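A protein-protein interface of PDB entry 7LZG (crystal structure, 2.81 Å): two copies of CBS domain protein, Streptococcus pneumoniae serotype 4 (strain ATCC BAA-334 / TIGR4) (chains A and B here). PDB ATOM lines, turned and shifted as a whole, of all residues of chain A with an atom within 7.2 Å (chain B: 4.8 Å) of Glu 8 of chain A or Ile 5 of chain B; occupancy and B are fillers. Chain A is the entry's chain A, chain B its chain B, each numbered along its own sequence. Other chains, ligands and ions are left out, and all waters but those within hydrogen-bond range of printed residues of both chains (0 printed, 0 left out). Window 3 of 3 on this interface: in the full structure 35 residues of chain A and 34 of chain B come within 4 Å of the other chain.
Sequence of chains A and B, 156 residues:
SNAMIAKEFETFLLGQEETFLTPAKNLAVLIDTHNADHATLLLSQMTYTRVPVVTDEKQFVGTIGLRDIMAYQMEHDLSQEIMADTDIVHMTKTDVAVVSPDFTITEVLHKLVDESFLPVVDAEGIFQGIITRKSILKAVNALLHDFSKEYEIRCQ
The side-chain hydroxyl of Thr 11 of chain A is in hydrogen-bond range of the backbone carbonyl oxygen of Glu 8 of chain A (2.8 Å).
Ile 5 of chain A touches Glu 8 of chain B, and with the chains exchanged Glu 8 of chain A touches Ile 5 of chain B. Ile 5 of chain A touches Phe 9 of chain B, but with the chains exchanged Phe 9 of chain A does not touch Ile 5 of chain B (5.9 Å). Phe 9 of chain B touches its own counterpart, Phe 9 of chain A. 7 positions are printed for both chains. Of the 9 pairs that touch across the chains among the printed residues, 3 have their exchanged pair printed and touching as well.
Printed residues of chain B within 4 Å of Glu 8 of chain A: Ile 5 (3.6 Å). Ile 5 of chain B touches just one residue of chain A: Glu 8. Of the printed residues of chain B, Leu 143 of chain A touches Ala 6 and Phe 9. Of the printed residues of chain B, Leu 144 of chain A touches Ala 6 and Phe 9. Leu 13 of chain A touches none of the printed residues of chain B. Glu 10 of chain A touches none of the printed residues of chain B. The nearest printed residue of chain B that does not touch Ile 5 of chain A is Ile 5 of chain B (4.1 Å).
Among the printed residues, merely in contact across the chains: Leu 143 of chain A with Ala 6 of chain B (3.5 Å), Phe 9 of chain A with Phe 9 of chain B (3.5 Å), Glu 8 of chain A with Ile 5 of chain B (3.6 Å), Leu 144 of chain A with Ala 6 of chain B (3.7 Å), Leu 143 of chain A with Phe 9 of chain B (3.7 Å), Ile 5 of chain A with Glu 8 of chain B (3.7 Å), Ile 5 of chain A with Phe 9 of chain B (3.8 Å), Asp 146 of chain A with Ala 3 of chain B (3.9 Å) and Leu 144 of chain A with Phe 9 of chain B (3.96 Å).
Hydrophobic or aromatic side chains of chain B that line the printed part of chain A: Ala 3, Ile 5, Ala 6 and Phe 9. Hydrophobic or aromatic side chains of chain A within 4 Å of the printed part of chain B: Ile 5, Phe 9, Leu 143 and Leu 144. Among the printed residues, 9 pairs touch across the chains. Among the printed residues, no Asp or Glu carboxylate lies within 4 Å of a Lys or Arg side-chain nitrogen of the other chain.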
ATOM      1  N   ALA A   3      10.081   2.237 -18.601  1.00  0.00           N
ATOM      2  CA  ALA A   3      10.186   3.645 -18.951  1.00  0.00           C
ATOM      3  C   ALA A   3       9.638   3.944 -20.336  1.00  0.00           C
ATOM      4  O   ALA A   3       9.253   5.089 -20.604  1.00  0.00           O
ATOM      5  CB  ALA A   3      11.644   4.107 -18.871  1.00  0.00           C
ATOM      6  N   MET A   4       9.596   2.949 -21.215  1.00  0.00           N
ATOM      7  CA  MET A   4       9.045   3.128 -22.547  1.00  0.00           C
ATOM      8  C   MET A   4       7.523   3.131 -22.483  1.00  0.00           C
ATOM      9  O   MET A   4       6.866   3.953 -23.122  1.00  0.00           O
ATOM     10  CB  MET A   4       9.538   2.028 -23.488  1.00  0.00           C
ATOM     11  CG  MET A   4       9.118   2.230 -24.930  1.00  0.00           C
ATOM     12  SD  MET A   4       9.767   3.919 -25.654  1.00  0.00           S
ATOM     13  CE  MET A   4       8.588   4.052 -27.199  1.00  0.00           C
ATOM     14  N   ILE A   5       6.967   2.205 -21.700  1.00  0.00           N
ATOM     15  CA  ILE A   5       5.520   2.170 -21.530  1.00  0.00           C
ATOM     16  C   ILE A   5       5.049   3.380 -20.729  1.00  0.00           C
ATOM     17  O   ILE A   5       3.948   3.893 -20.959  1.00  0.00           O
ATOM     18  CB  ILE A   5       5.088   0.837 -20.885  1.00  0.00           C
ATOM     19  CG1 ILE A   5       3.562   0.739 -20.825  1.00  0.00           C
ATOM     20  CG2 ILE A   5       5.705   0.665 -19.504  1.00  0.00           C
ATOM     21  CD1 ILE A   5       2.895   0.808 -22.183  1.00  0.00           C
ATOM     22  N   ALA A   6       5.873   3.869 -19.797  1.00  0.00           N
ATOM     23  CA  ALA A   6       5.521   5.078 -19.062  1.00  0.00           C
ATOM     24  C   ALA A   6       5.472   6.292 -19.979  1.00  0.00           C
ATOM     25  O   ALA A   6       4.654   7.195 -19.768  1.00  0.00           O
ATOM     26  CB  ALA A   6       6.510   5.313 -17.921  1.00  0.00           C
ATOM     27  N   LYS A   7       6.336   6.336 -20.995  1.00  0.00           N
ATOM     28  CA  LYS A   7       6.287   7.439 -21.949  1.00  0.00           C
ATOM     29  C   LYS A   7       5.064   7.325 -22.850  1.00  0.00           C
ATOM     30  O   LYS A   7       4.401   8.329 -23.137  1.00  0.00           O
ATOM     31  CB  LYS A   7       7.574   7.475 -22.774  1.00  0.00           C
ATOM     32  CG  LYS A   7       7.689   8.668 -23.710  1.00  0.00           C
ATOM     33  CD  LYS A   7       7.330   8.298 -25.143  1.00  0.00           C
ATOM     34  CE  LYS A   7       7.354   9.519 -26.048  1.00  0.00           C
ATOM     35  NZ  LYS A   7       8.674  10.205 -26.009  1.00  0.00           N
ATOM     36  N   GLU A   8       4.749   6.109 -23.302  1.00  0.00           N
ATOM     37  CA  GLU A   8       3.562   5.911 -24.128  1.00  0.00           C
ATOM     38  C   GLU A   8       2.287   6.185 -23.338  1.00  0.00           C
ATOM     39  O   GLU A   8       1.317   6.724 -23.882  1.00  0.00           O
ATOM     40  CB  GLU A   8       3.551   4.492 -24.694  1.00  0.00           C
ATOM     41  CG  GLU A   8       4.719   4.184 -25.615  1.00  0.00           C
ATOM     42  CD  GLU A   8       4.791   2.718 -25.995  1.00  0.00           C
ATOM     43  OE1 GLU A   8       4.164   1.889 -25.301  1.00  0.00           O
ATOM     44  OE2 GLU A   8       5.474   2.394 -26.988  1.00  0.00           O
ATOM     45  N   PHE A   9       2.271   5.821 -22.052  1.00  0.00           N
ATOM     46  CA  PHE A   9       1.097   6.076 -21.224  1.00  0.00           C
ATOM     47  C   PHE A   9       0.904   7.568 -20.985  1.00  0.00           C
ATOM     48  O   PHE A   9      -0.232   8.053 -20.938  1.00  0.00           O
ATOM     49  CB  PHE A   9       1.220   5.324 -19.898  1.00  0.00           C
ATOM     50  CG  PHE A   9       0.078   5.563 -18.948  1.00  0.00           C
ATOM     51  CD1 PHE A   9      -1.224   5.270 -19.315  1.00  0.00           C
ATOM     52  CD2 PHE A   9       0.312   6.059 -17.675  1.00  0.00           C
ATOM     53  CE1 PHE A   9      -2.274   5.483 -18.437  1.00  0.00           C
ATOM     54  CE2 PHE A   9      -0.732   6.272 -16.792  1.00  0.00           C
ATOM     55  CZ  PHE A   9      -2.027   5.984 -17.174  1.00  0.00           C
ATOM     56  N   GLU A  10       2.003   8.312 -20.838  1.00  0.00           N
ATOM     57  CA  GLU A  10       1.896   9.751 -20.624  1.00  0.00           C
ATOM     58  C   GLU A  10       1.382  10.461 -21.870  1.00  0.00           C
ATOM     59  O   GLU A  10       0.507  11.328 -21.777  1.00  0.00           O
ATOM     60  CB  GLU A  10       3.250  10.321 -20.207  1.00  0.00           C
ATOM     61  CG  GLU A  10       3.245  11.821 -19.978  1.00  0.00           C
ATOM     62  CD  GLU A  10       4.577  12.330 -19.464  1.00  0.00           C
ATOM     63  OE1 GLU A  10       5.492  11.505 -19.264  1.00  0.00           O
ATOM     64  OE2 GLU A  10       4.708  13.555 -19.259  1.00  0.00           O
ATOM     65  N   THR A  11       1.911  10.105 -23.043  1.00  0.00           N
ATOM     66  CA  THR A  11       1.487  10.762 -24.274  1.00  0.00           C
ATOM     67  C   THR A  11       0.005  10.531 -24.542  1.00  0.00           C
ATOM     68  O   THR A  11      -0.692  11.426 -25.032  1.00  0.00           O
ATOM     69  CB  THR A  11       2.330  10.272 -25.451  1.00  0.00           C
ATOM     70  OG1 THR A  11       2.357   8.840 -25.458  1.00  0.00           O
ATOM     71  CG2 THR A  11       3.754  10.802 -25.340  1.00  0.00           C
ATOM     72  N   PHE A  12      -0.498   9.338 -24.214  1.00  0.00           N
ATOM     73  CA  PHE A  12      -1.923   9.075 -24.380  1.00  0.00           C
ATOM     74  C   PHE A  12      -2.763   9.903 -23.414  1.00  0.00           C
ATOM     75  O   PHE A  12      -3.885  10.296 -23.753  1.00  0.00           O
ATOM     76  CB  PHE A  12      -2.207   7.583 -24.195  1.00  0.00           C
ATOM     77  CG  PHE A  12      -3.657   7.216 -24.354  1.00  0.00           C
ATOM     78  CD1 PHE A  12      -4.202   7.022 -25.613  1.00  0.00           C
ATOM     79  CD2 PHE A  12      -4.473   7.060 -23.246  1.00  0.00           C
ATOM     80  CE1 PHE A  12      -5.534   6.685 -25.763  1.00  0.00           C
ATOM     81  CE2 PHE A  12      -5.805   6.722 -23.390  1.00  0.00           C
ATOM     82  CZ  PHE A  12      -6.336   6.533 -24.650  1.00  0.00           C
ATOM     83  N   LEU A  13      -2.240  10.181 -22.216  1.00  0.00           N
ATOM     84  CA  LEU A  13      -2.999  10.962 -21.244  1.00  0.00           C
ATOM     85  C   LEU A  13      -3.137  12.414 -21.683  1.00  0.00           C
ATOM     86  O   LEU A  13      -4.169  13.047 -21.432  1.00  0.00           O
ATOM     87  CB  LEU A  13      -2.340  10.876 -19.869  1.00  0.00           C
ATOM     88  CG  LEU A  13      -2.517   9.546 -19.138  1.00  0.00           C
ATOM     89  CD1 LEU A  13      -1.824   9.579 -17.788  1.00  0.00           C
ATOM     90  CD2 LEU A  13      -3.994   9.222 -18.979  1.00  0.00           C
ATOM     91  N   LEU A 143      -7.180   2.931 -22.858  1.00  0.00           N
ATOM     92  CA  LEU A 143      -5.897   2.510 -23.408  1.00  0.00           C
ATOM     93  C   LEU A 143      -5.873   1.019 -23.717  1.00  0.00           C
ATOM     94  O   LEU A 143      -5.143   0.589 -24.617  1.00  0.00           O
ATOM     95  CB  LEU A 143      -4.770   2.866 -22.436  1.00  0.00           C
ATOM     96  CG  LEU A 143      -3.337   2.667 -22.930  1.00  0.00           C
ATOM     97  CD1 LEU A 143      -3.065   3.550 -24.135  1.00  0.00           C
ATOM     98  CD2 LEU A 143      -2.346   2.953 -21.817  1.00  0.00           C
ATOM     99  N   LEU A 144      -6.657   0.221 -22.991  1.00  0.00           N
ATOM    100  CA  LEU A 144      -6.713  -1.215 -23.232  1.00  0.00           C
ATOM    101  C   LEU A 144      -7.591  -1.584 -24.421  1.00  0.00           C
ATOM    102  O   LEU A 144      -7.603  -2.754 -24.819  1.00  0.00           O
ATOM    103  CB  LEU A 144      -7.217  -1.938 -21.980  1.00  0.00           C
ATOM    104  CG  LEU A 144      -6.367  -1.813 -20.713  1.00  0.00           C
ATOM    105  CD1 LEU A 144      -7.041  -2.526 -19.553  1.00  0.00           C
ATOM    106  CD2 LEU A 144      -4.969  -2.365 -20.939  1.00  0.00           C
ATOM    107  N   ASP A 146      -7.714  -0.194 -27.950  1.00  0.00           N
ATOM    108  CA  ASP A 146      -7.194   0.677 -28.996  1.00  0.00           C
ATOM    109  C   ASP A 146      -6.447  -0.140 -30.045  1.00  0.00           C
ATOM    110  O   ASP A 146      -6.865  -1.243 -30.398  1.00  0.00           O
ATOM    111  CB  ASP A 146      -6.276   1.744 -28.393  1.00  0.00           C
ATOM    112  CG  ASP A 146      -6.096   2.948 -29.301  1.00  0.00           C
ATOM    113  OD1 ASP A 146      -6.183   2.789 -30.537  1.00  0.00           O
ATOM    114  OD2 ASP A 146      -5.866   4.058 -28.775  1.00  0.00           O
ATOM    115  N   ASN B   2      -0.485   1.664 -31.781  1.00  0.00           N
ATOM    116  CA  ASN B   2      -0.414   0.224 -31.996  1.00  0.00           C
ATOM    117  C   ASN B   2      -1.180  -0.521 -30.906  1.00  0.00           C
ATOM    118  O   ASN B   2      -1.104  -0.166 -29.729  1.00  0.00           O
ATOM    119  CB  ASN B   2       1.043  -0.245 -32.032  1.00  0.00           C
ATOM    120  CG  ASN B   2       1.201  -1.633 -32.628  1.00  0.00           C
ATOM    121  OD1 ASN B   2       0.223  -2.356 -32.823  1.00  0.00           O
ATOM    122  ND2 ASN B   2       2.440  -2.015 -32.915  1.00  0.00           N
ATOM    123  N   ALA B   3      -1.916  -1.560 -31.305  1.00  0.00           N
ATOM    124  CA  ALA B   3      -2.627  -2.405 -30.352  1.00  0.00           C
ATOM    125  C   ALA B   3      -1.692  -3.258 -29.506  1.00  0.00           C
ATOM    126  O   ALA B   3      -2.167  -3.975 -28.618  1.00  0.00           O
ATOM    127  CB  ALA B   3      -3.623  -3.303 -31.089  1.00  0.00           C
ATOM    128  N   MET B   4      -0.389  -3.203 -29.763  1.00  0.00           N
ATOM    129  CA  MET B   4       0.605  -3.903 -28.963  1.00  0.00           C
ATOM    130  C   MET B   4       0.847  -3.155 -27.653  1.00  0.00           C
ATOM    131  O   MET B   4       1.313  -3.730 -26.668  1.00  0.00           O
ATOM    132  CB  MET B   4       1.908  -4.048 -29.755  1.00  0.00           C
ATOM    133  CG  MET B   4       3.011  -4.830 -29.061  1.00  0.00           C
ATOM    134  SD  MET B   4       2.714  -6.753 -29.005  1.00  0.00           S
ATOM    135  CE  MET B   4       4.487  -7.306 -28.410  1.00  0.00           C
ATOM    136  N   ILE B   5       0.517  -1.860 -27.651  1.00  0.00           N
ATOM    137  CA  ILE B   5       0.708  -1.040 -26.459  1.00  0.00           C
ATOM    138  C   ILE B   5      -0.230  -1.486 -25.345  1.00  0.00           C
ATOM    139  O   ILE B   5       0.157  -1.527 -24.170  1.00  0.00           O
ATOM    140  CB  ILE B   5       0.516   0.448 -26.804  1.00  0.00           C
ATOM    141  CG1 ILE B   5       1.547   0.885 -27.845  1.00  0.00           C
ATOM    142  CG2 ILE B   5       0.616   1.308 -25.553  1.00  0.00           C
ATOM    143  CD1 ILE B   5       1.450   2.345 -28.229  1.00  0.00           C
ATOM    144  N   ALA B   6      -1.473  -1.830 -25.690  1.00  0.00           N
ATOM    145  CA  ALA B   6      -2.415  -2.315 -24.686  1.00  0.00           C
ATOM    146  C   ALA B   6      -1.918  -3.594 -24.026  1.00  0.00           C
ATOM    147  O   ALA B   6      -2.170  -3.816 -22.836  1.00  0.00           O
ATOM    148  CB  ALA B   6      -3.789  -2.538 -25.315  1.00  0.00           C
ATOM    149  N   LYS B   7      -1.219  -4.445 -24.777  1.00  0.00           N
ATOM    150  CA  LYS B   7      -0.574  -5.604 -24.169  1.00  0.00           C
ATOM    151  C   LYS B   7       0.545  -5.173 -23.228  1.00  0.00           C
ATOM    152  O   LYS B   7       0.687  -5.726 -22.130  1.00  0.00           O
ATOM    153  CB  LYS B   7      -0.031  -6.536 -25.254  1.00  0.00           C
ATOM    154  CG  LYS B   7      -1.085  -7.350 -25.994  1.00  0.00           C
ATOM    155  CD  LYS B   7      -0.492  -7.974 -27.254  1.00  0.00           C
ATOM    156  CE  LYS B   7      -1.363  -9.092 -27.810  1.00  0.00           C
ATOM    157  NZ  LYS B   7      -1.308 -10.317 -26.961  1.00  0.00           N
ATOM    158  N   GLU B   8       1.347  -4.186 -23.639  1.00  0.00           N
ATOM    159  CA  GLU B   8       2.437  -3.708 -22.794  1.00  0.00           C
ATOM    160  C   GLU B   8       1.909  -3.124 -21.490  1.00  0.00           C
ATOM    161  O   GLU B   8       2.454  -3.394 -20.414  1.00  0.00           O
ATOM    162  CB  GLU B   8       3.266  -2.664 -23.542  1.00  0.00           C
ATOM    163  CG  GLU B   8       3.948  -3.167 -24.808  1.00  0.00           C
ATOM    164  CD  GLU B   8       5.250  -3.900 -24.531  1.00  0.00           C
ATOM    165  OE1 GLU B   8       5.580  -4.120 -23.346  1.00  0.00           O
ATOM    166  OE2 GLU B   8       5.944  -4.259 -25.505  1.00  0.00           O
ATOM    167  N   PHE B   9       0.848  -2.320 -21.569  1.00  0.00           N
ATOM    168  CA  PHE B   9       0.303  -1.695 -20.370  1.00  0.00           C
ATOM    169  C   PHE B   9      -0.350  -2.725 -19.457  1.00  0.00           C
ATOM    170  O   PHE B   9      -0.218  -2.646 -18.230  1.00  0.00           O
ATOM    171  CB  PHE B   9      -0.698  -0.608 -20.756  1.00  0.00           C
ATOM    172  CG  PHE B   9      -1.182   0.208 -19.595  1.00  0.00           C
ATOM    173  CD1 PHE B   9      -0.420   1.256 -19.105  1.00  0.00           C
ATOM    174  CD2 PHE B   9      -2.398  -0.068 -18.995  1.00  0.00           C
ATOM    175  CE1 PHE B   9      -0.861   2.011 -18.035  1.00  0.00           C
ATOM    176  CE2 PHE B   9      -2.846   0.684 -17.925  1.00  0.00           C
ATOM    177  CZ  PHE B   9      -2.075   1.724 -17.445  1.00  0.00           C
